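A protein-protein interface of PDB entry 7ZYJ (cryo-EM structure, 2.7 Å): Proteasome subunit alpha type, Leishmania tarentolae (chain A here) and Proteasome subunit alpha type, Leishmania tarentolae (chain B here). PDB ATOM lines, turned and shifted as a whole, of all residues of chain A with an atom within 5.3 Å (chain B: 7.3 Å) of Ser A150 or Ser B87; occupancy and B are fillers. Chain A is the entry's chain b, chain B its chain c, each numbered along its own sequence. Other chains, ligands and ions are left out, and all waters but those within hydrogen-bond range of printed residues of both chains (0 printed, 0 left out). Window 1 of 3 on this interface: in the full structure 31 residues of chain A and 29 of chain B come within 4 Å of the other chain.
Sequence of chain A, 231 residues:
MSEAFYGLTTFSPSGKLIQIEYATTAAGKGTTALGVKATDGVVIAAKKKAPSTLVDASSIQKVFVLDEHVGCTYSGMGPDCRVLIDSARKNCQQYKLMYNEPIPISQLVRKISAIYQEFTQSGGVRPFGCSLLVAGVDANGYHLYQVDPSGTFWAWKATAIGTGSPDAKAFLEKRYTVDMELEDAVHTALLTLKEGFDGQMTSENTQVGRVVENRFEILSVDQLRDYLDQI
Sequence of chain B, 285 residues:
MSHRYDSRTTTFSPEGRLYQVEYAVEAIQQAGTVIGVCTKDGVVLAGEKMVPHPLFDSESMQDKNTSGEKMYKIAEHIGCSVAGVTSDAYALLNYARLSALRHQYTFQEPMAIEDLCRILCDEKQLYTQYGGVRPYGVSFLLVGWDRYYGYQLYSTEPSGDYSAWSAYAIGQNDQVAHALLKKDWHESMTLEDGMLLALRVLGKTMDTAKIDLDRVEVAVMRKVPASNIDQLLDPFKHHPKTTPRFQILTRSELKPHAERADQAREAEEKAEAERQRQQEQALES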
ATOM      1  N   ILE A  20     -20.668 -33.520 -30.197  1.00  0.00           N
ATOM      2  CA  ILE A  20     -21.900 -33.605 -29.420  1.00  0.00           C
ATOM      3  C   ILE A  20     -22.453 -35.024 -29.444  1.00  0.00           C
ATOM      4  O   ILE A  20     -22.987 -35.512 -28.442  1.00  0.00           O
ATOM      5  CB  ILE A  20     -22.927 -32.581 -29.937  1.00  0.00           C
ATOM      6  CG1 ILE A  20     -22.357 -31.166 -29.836  1.00  0.00           C
ATOM      7  CG2 ILE A  20     -24.226 -32.688 -29.163  1.00  0.00           C
ATOM      8  CD1 ILE A  20     -23.333 -30.087 -30.235  1.00  0.00           C
ATOM      9  N   THR A  24     -23.082 -37.382 -26.253  1.00  0.00           N
ATOM     10  CA  THR A  24     -24.330 -38.100 -26.017  1.00  0.00           C
ATOM     11  C   THR A  24     -24.073 -39.583 -25.786  1.00  0.00           C
ATOM     12  O   THR A  24     -24.722 -40.209 -24.941  1.00  0.00           O
ATOM     13  CB  THR A  24     -25.281 -37.899 -27.198  1.00  0.00           C
ATOM     14  OG1 THR A  24     -25.396 -36.501 -27.488  1.00  0.00           O
ATOM     15  CG2 THR A  24     -26.658 -38.458 -26.876  1.00  0.00           C
ATOM     16  N   SER A 113     -30.290 -25.731 -20.054  1.00  0.00           N
ATOM     17  CA  SER A 113     -30.024 -25.972 -21.466  1.00  0.00           C
ATOM     18  C   SER A 113     -29.073 -24.946 -22.069  1.00  0.00           C
ATOM     19  O   SER A 113     -28.356 -25.273 -23.019  1.00  0.00           O
ATOM     20  CB  SER A 113     -31.337 -25.983 -22.247  1.00  0.00           C
ATOM     21  OG  SER A 113     -31.101 -25.934 -23.642  1.00  0.00           O
ATOM     22  N   TYR A 116     -25.414 -26.045 -21.479  1.00  0.00           N
ATOM     23  CA  TYR A 116     -25.093 -27.106 -22.428  1.00  0.00           C
ATOM     24  C   TYR A 116     -24.688 -26.530 -23.778  1.00  0.00           C
ATOM     25  O   TYR A 116     -23.650 -26.897 -24.338  1.00  0.00           O
ATOM     26  CB  TYR A 116     -26.296 -28.035 -22.589  1.00  0.00           C
ATOM     27  CG  TYR A 116     -26.358 -29.179 -21.607  1.00  0.00           C
ATOM     28  CD1 TYR A 116     -25.442 -30.218 -21.664  1.00  0.00           C
ATOM     29  CD2 TYR A 116     -27.342 -29.228 -20.631  1.00  0.00           C
ATOM     30  CE1 TYR A 116     -25.503 -31.271 -20.773  1.00  0.00           C
ATOM     31  CE2 TYR A 116     -27.406 -30.274 -19.735  1.00  0.00           C
ATOM     32  CZ  TYR A 116     -26.487 -31.294 -19.813  1.00  0.00           C
ATOM     33  OH  TYR A 116     -26.553 -32.339 -18.922  1.00  0.00           O
ATOM     34  N   GLN A 117     -25.500 -25.618 -24.314  1.00  0.00           N
ATOM     35  CA  GLN A 117     -25.176 -24.992 -25.592  1.00  0.00           C
ATOM     36  C   GLN A 117     -23.884 -24.193 -25.498  1.00  0.00           C
ATOM     37  O   GLN A 117     -23.062 -24.209 -26.424  1.00  0.00           O
ATOM     38  CB  GLN A 117     -26.329 -24.098 -26.043  1.00  0.00           C
ATOM     39  CG  GLN A 117     -26.348 -23.814 -27.532  1.00  0.00           C
ATOM     40  CD  GLN A 117     -25.592 -22.557 -27.896  1.00  0.00           C
ATOM     41  OE1 GLN A 117     -25.476 -21.633 -27.092  1.00  0.00           O
ATOM     42  NE2 GLN A 117     -25.076 -22.512 -29.117  1.00  0.00           N
ATOM     43  N   THR A 120     -21.150 -26.560 -25.789  1.00  0.00           N
ATOM     44  CA  THR A 120     -21.097 -27.183 -27.106  1.00  0.00           C
ATOM     45  C   THR A 120     -20.716 -26.212 -28.214  1.00  0.00           C
ATOM     46  O   THR A 120     -20.510 -26.651 -29.349  1.00  0.00           O
ATOM     47  CB  THR A 120     -22.437 -27.834 -27.466  1.00  0.00           C
ATOM     48  OG1 THR A 120     -23.467 -26.839 -27.497  1.00  0.00           O
ATOM     49  CG2 THR A 120     -22.798 -28.928 -26.475  1.00  0.00           C
ATOM     50  N   ASP A 148     -30.378 -33.348 -22.627  1.00  0.00           N
ATOM     51  CA  ASP A 148     -29.284 -34.074 -23.250  1.00  0.00           C
ATOM     52  C   ASP A 148     -28.071 -33.168 -23.435  1.00  0.00           C
ATOM     53  O   ASP A 148     -28.178 -31.944 -23.310  1.00  0.00           O
ATOM     54  CB  ASP A 148     -29.727 -34.649 -24.604  1.00  0.00           C
ATOM     55  CG  ASP A 148     -30.328 -36.034 -24.474  1.00  0.00           C
ATOM     56  OD1 ASP A 148     -30.024 -36.720 -23.477  1.00  0.00           O
ATOM     57  OD2 ASP A 148     -31.094 -36.444 -25.370  1.00  0.00           O
ATOM     58  N   PRO A 149     -26.894 -33.740 -23.717  1.00  0.00           N
ATOM     59  CA  PRO A 149     -25.696 -32.901 -23.895  1.00  0.00           C
ATOM     60  C   PRO A 149     -25.811 -31.870 -25.005  1.00  0.00           C
ATOM     61  O   PRO A 149     -25.104 -30.857 -24.956  1.00  0.00           O
ATOM     62  CB  PRO A 149     -24.595 -33.925 -24.196  1.00  0.00           C
ATOM     63  CG  PRO A 149     -25.050 -35.158 -23.527  1.00  0.00           C
ATOM     64  CD  PRO A 149     -26.545 -35.171 -23.650  1.00  0.00           C
ATOM     65  N   SER A 150     -26.663 -32.089 -26.008  1.00  0.00           N
ATOM     66  CA  SER A 150     -26.823 -31.095 -27.062  1.00  0.00           C
ATOM     67  C   SER A 150     -27.545 -29.847 -26.574  1.00  0.00           C
ATOM     68  O   SER A 150     -27.518 -28.823 -27.264  1.00  0.00           O
ATOM     69  CB  SER A 150     -27.582 -31.691 -28.247  1.00  0.00           C
ATOM     70  OG  SER A 150     -28.905 -32.039 -27.882  1.00  0.00           O
ATOM     71  N   GLY A 151     -28.174 -29.904 -25.403  1.00  0.00           N
ATOM     72  CA  GLY A 151     -28.975 -28.815 -24.894  1.00  0.00           C
ATOM     73  C   GLY A 151     -30.459 -28.961 -25.146  1.00  0.00           C
ATOM     74  O   GLY A 151     -31.247 -28.210 -24.559  1.00  0.00           O
ATOM     75  N   THR A 152     -30.860 -29.901 -25.995  1.00  0.00           N
ATOM     76  CA  THR A 152     -32.273 -30.123 -26.259  1.00  0.00           C
ATOM     77  C   THR A 152     -32.951 -30.723 -25.034  1.00  0.00           C
ATOM     78  O   THR A 152     -32.387 -31.579 -24.348  1.00  0.00           O
ATOM     79  CB  THR A 152     -32.447 -31.045 -27.465  1.00  0.00           C
ATOM     80  OG1 THR A 152     -31.675 -30.546 -28.563  1.00  0.00           O
ATOM     81  CG2 THR A 152     -33.907 -31.112 -27.881  1.00  0.00           C
ATOM     82  N   GLY B  84     -33.005 -26.404 -37.813  1.00  0.00           N
ATOM     83  CA  GLY B  84     -31.615 -26.716 -37.553  1.00  0.00           C
ATOM     84  C   GLY B  84     -31.354 -27.103 -36.113  1.00  0.00           C
ATOM     85  O   GLY B  84     -32.165 -27.796 -35.493  1.00  0.00           O
ATOM     86  N   VAL B  85     -30.222 -26.660 -35.571  1.00  0.00           N
ATOM     87  CA  VAL B  85     -29.877 -26.933 -34.181  1.00  0.00           C
ATOM     88  C   VAL B  85     -30.814 -26.137 -33.284  1.00  0.00           C
ATOM     89  O   VAL B  85     -30.711 -24.908 -33.195  1.00  0.00           O
ATOM     90  CB  VAL B  85     -28.405 -26.591 -33.893  1.00  0.00           C
ATOM     91  CG1 VAL B  85     -28.011 -27.062 -32.504  1.00  0.00           C
ATOM     92  CG2 VAL B  85     -27.501 -27.207 -34.949  1.00  0.00           C
ATOM     93  N   THR B  86     -31.741 -26.833 -32.621  1.00  0.00           N
ATOM     94  CA  THR B  86     -32.728 -26.151 -31.790  1.00  0.00           C
ATOM     95  C   THR B  86     -32.070 -25.439 -30.616  1.00  0.00           C
ATOM     96  O   THR B  86     -32.468 -24.324 -30.256  1.00  0.00           O
ATOM     97  CB  THR B  86     -33.774 -27.149 -31.291  1.00  0.00           C
ATOM     98  OG1 THR B  86     -33.254 -27.862 -30.162  1.00  0.00           O
ATOM     99  CG2 THR B  86     -34.127 -28.138 -32.388  1.00  0.00           C
ATOM    100  N   SER B  87     -31.064 -26.066 -30.006  1.00  0.00           N
ATOM    101  CA  SER B  87     -30.359 -25.431 -28.902  1.00  0.00           C
ATOM    102  C   SER B  87     -29.620 -24.175 -29.345  1.00  0.00           C
ATOM    103  O   SER B  87     -29.539 -23.215 -28.572  1.00  0.00           O
ATOM    104  CB  SER B  87     -29.387 -26.422 -28.264  1.00  0.00           C
ATOM    105  OG  SER B  87     -28.776 -25.869 -27.114  1.00  0.00           O
ATOM    106  N   ASP B  88     -29.082 -24.161 -30.566  1.00  0.00           N
ATOM    107  CA  ASP B  88     -28.546 -22.923 -31.120  1.00  0.00           C
ATOM    108  C   ASP B  88     -29.656 -21.925 -31.414  1.00  0.00           C
ATOM    109  O   ASP B  88     -29.440 -20.712 -31.320  1.00  0.00           O
ATOM    110  CB  ASP B  88     -27.751 -23.210 -32.394  1.00  0.00           C
ATOM    111  CG  ASP B  88     -26.398 -23.825 -32.111  1.00  0.00           C
ATOM    112  OD1 ASP B  88     -25.901 -23.678 -30.975  1.00  0.00           O
ATOM    113  OD2 ASP B  88     -25.827 -24.452 -33.028  1.00  0.00           O
ATOM    114  N   ALA B  89     -30.842 -22.415 -31.780  1.00  0.00           N
ATOM    115  CA  ALA B  89     -31.952 -21.526 -32.096  1.00  0.00           C
ATOM    116  C   ALA B  89     -32.472 -20.803 -30.861  1.00  0.00           C
ATOM    117  O   ALA B  89     -32.925 -19.660 -30.966  1.00  0.00           O
ATOM    118  CB  ALA B  89     -33.081 -22.310 -32.760  1.00  0.00           C
ATOM    119  N   TYR B  90     -32.431 -21.451 -29.695  1.00  0.00           N
ATOM    120  CA  TYR B  90     -32.947 -20.816 -28.482  1.00  0.00           C
ATOM    121  C   TYR B  90     -32.138 -19.580 -28.105  1.00  0.00           C
ATOM    122  O   TYR B  90     -32.707 -18.551 -27.721  1.00  0.00           O
ATOM    123  CB  TYR B  90     -32.964 -21.816 -27.326  1.00  0.00           C
ATOM    124  CG  TYR B  90     -34.173 -22.722 -27.318  1.00  0.00           C
ATOM    125  CD1 TYR B  90     -35.415 -22.249 -26.920  1.00  0.00           C
ATOM    126  CD2 TYR B  90     -34.071 -24.053 -27.697  1.00  0.00           C
ATOM    127  CE1 TYR B  90     -36.523 -23.072 -26.909  1.00  0.00           C
ATOM    128  CE2 TYR B  90     -35.171 -24.884 -27.689  1.00  0.00           C
ATOM    129  CZ  TYR B  90     -36.395 -24.389 -27.294  1.00  0.00           C
ATOM    130  OH  TYR B  90     -37.496 -25.214 -27.284  1.00  0.00           O
ATOM    131  N   ALA B  91     -30.808 -19.664 -28.200  1.00  0.00           N
ATOM    132  CA  ALA B  91     -29.966 -18.520 -27.863  1.00  0.00           C
ATOM    133  C   ALA B  91     -30.229 -17.350 -28.802  1.00  0.00           C
ATOM    134  O   ALA B  91     -30.332 -16.196 -28.368  1.00  0.00           O
ATOM    135  CB  ALA B  91     -28.493 -18.926 -27.902  1.00  0.00           C
ATOM    136  N   LEU B  92     -30.346 -17.631 -30.101  1.00  0.00           N
ATOM    137  CA  LEU B  92     -30.631 -16.571 -31.060  1.00  0.00           C
ATOM    138  C   LEU B  92     -32.028 -15.999 -30.868  1.00  0.00           C
ATOM    139  O   LEU B  92     -32.233 -14.799 -31.068  1.00  0.00           O
ATOM    140  CB  LEU B  92     -30.451 -17.090 -32.485  1.00  0.00           C
ATOM    141  CG  LEU B  92     -28.997 -17.264 -32.925  1.00  0.00           C
ATOM    142  CD1 LEU B  92     -28.920 -17.713 -34.371  1.00  0.00           C
ATOM    143  CD2 LEU B  92     -28.217 -15.975 -32.721  1.00  0.00           C
ATOM    144  N   ARG B 134     -17.416 -22.408 -33.921  1.00  0.00           N
ATOM    145  CA  ARG B 134     -18.352 -22.796 -34.963  1.00  0.00           C
ATOM    146  C   ARG B 134     -19.501 -21.791 -35.047  1.00  0.00           C
ATOM    147  O   ARG B 134     -19.858 -21.155 -34.052  1.00  0.00           O
ATOM    148  CB  ARG B 134     -18.901 -24.195 -34.694  1.00  0.00           C
ATOM    149  CG  ARG B 134     -19.867 -24.277 -33.525  1.00  0.00           C
ATOM    150  CD  ARG B 134     -20.623 -25.593 -33.529  1.00  0.00           C
ATOM    151  NE  ARG B 134     -21.478 -25.739 -32.359  1.00  0.00           N
ATOM    152  CZ  ARG B 134     -22.692 -25.216 -32.248  1.00  0.00           C
ATOM    153  NH1 ARG B 134     -23.227 -24.500 -33.223  1.00  0.00           N
ATOM    154  NH2 ARG B 134     -23.387 -25.418 -31.133  1.00  0.00           N
ATOM    155  N   TYR B 136     -23.604 -20.640 -35.912  1.00  0.00           N
ATOM    156  CA  TYR B 136     -24.913 -21.174 -35.562  1.00  0.00           C
ATOM    157  C   TYR B 136     -25.454 -21.984 -36.734  1.00  0.00           C
ATOM    158  O   TYR B 136     -25.503 -21.490 -37.864  1.00  0.00           O
ATOM    159  CB  TYR B 136     -25.877 -20.046 -35.205  1.00  0.00           C
ATOM    160  CG  TYR B 136     -25.467 -19.226 -34.006  1.00  0.00           C
ATOM    161  CD1 TYR B 136     -25.802 -19.625 -32.720  1.00  0.00           C
ATOM    162  CD2 TYR B 136     -24.757 -18.045 -34.160  1.00  0.00           C
ATOM    163  CE1 TYR B 136     -25.434 -18.876 -31.621  1.00  0.00           C
ATOM    164  CE2 TYR B 136     -24.384 -17.289 -33.069  1.00  0.00           C
ATOM    165  CZ  TYR B 136     -24.726 -17.708 -31.802  1.00  0.00           C
ATOM    166  OH  TYR B 136     -24.356 -16.957 -30.712  1.00  0.00           O
ATOM    167  N   VAL B 138     -28.523 -22.818 -37.772  1.00  0.00           N
ATOM    168  CA  VAL B 138     -29.969 -22.632 -37.712  1.00  0.00           C
ATOM    169  C   VAL B 138     -30.385 -21.608 -38.760  1.00  0.00           C
ATOM    170  O   VAL B 138     -29.663 -20.644 -39.032  1.00  0.00           O
ATOM    171  CB  VAL B 138     -30.420 -22.215 -36.295  1.00  0.00           C
ATOM    172  CG1 VAL B 138     -29.859 -20.853 -35.928  1.00  0.00           C
ATOM    173  CG2 VAL B 138     -31.936 -22.216 -36.195  1.00  0.00           C
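Printed residues of chain B that touch a printed residue of chain A: Thr B86, Ser B87, Asp B88 and Arg B134.
Along chain A the printed residues that touch a printed residue of chain B span positions 117 to 152.
Among the printed residues, 7 pairs touch across the chains.
The side-chain hydroxyl (OG) of Ser A113 is in hydrogen-bond range of the backbone carbonyl oxygen (O) of Gly A151.
The backbone carbonyl oxygen (O) of Tyr A116 lies close to the side-chain hydroxyl (OG1) of Thr A120 (3.2 Å).
The guanidinium group of Arg B134 is in salt-bridge range of the side-chain carboxylate of Asp B88.
The side-chain hydroxyl (OG) of Ser A150 lies within hydrogen-bond range of the side-chain hydroxyl (OG1) of Thr A152 (3.2 Å).
O of Gln A117 sits at hydrogen-bond distance from OG1 of Thr A120.
The side-chain amide nitrogen of Gln A117 sits close to the side-chain carboxylate of Asp B88, 2.3 Å away.
NE of Arg B134 sits at hydrogen-bond distance from O of Thr A120 (3.3 Å).
OG of Ser B87 sits close to O of Ser A150, 3.2 Å away.
Ser A150 touches one residue of chain B.
Printed residues of chain B within 4 Å of Thr A152: Thr B86 (3.5 Å).
Of the printed residues of chain A, Thr B86 touches Thr A152 (3.5 Å).
Ser B87 touches three residues of chain A.
The nearest residue of chain A that does not touch Ser B87 is Ser A113 (4.2 Å).
The nearest printed residue of chain B that does not touch Gly A151 is Thr B86 (5.8 Å).
OG of Ser B87 touches CB of Gln A117, 3.2 Å away.
Gln A117 touches Arg B134.
Gly A151 touches Ser B87.
OG1 of Thr A152 touches OG1 of Thr B86, at 3.5 Å.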
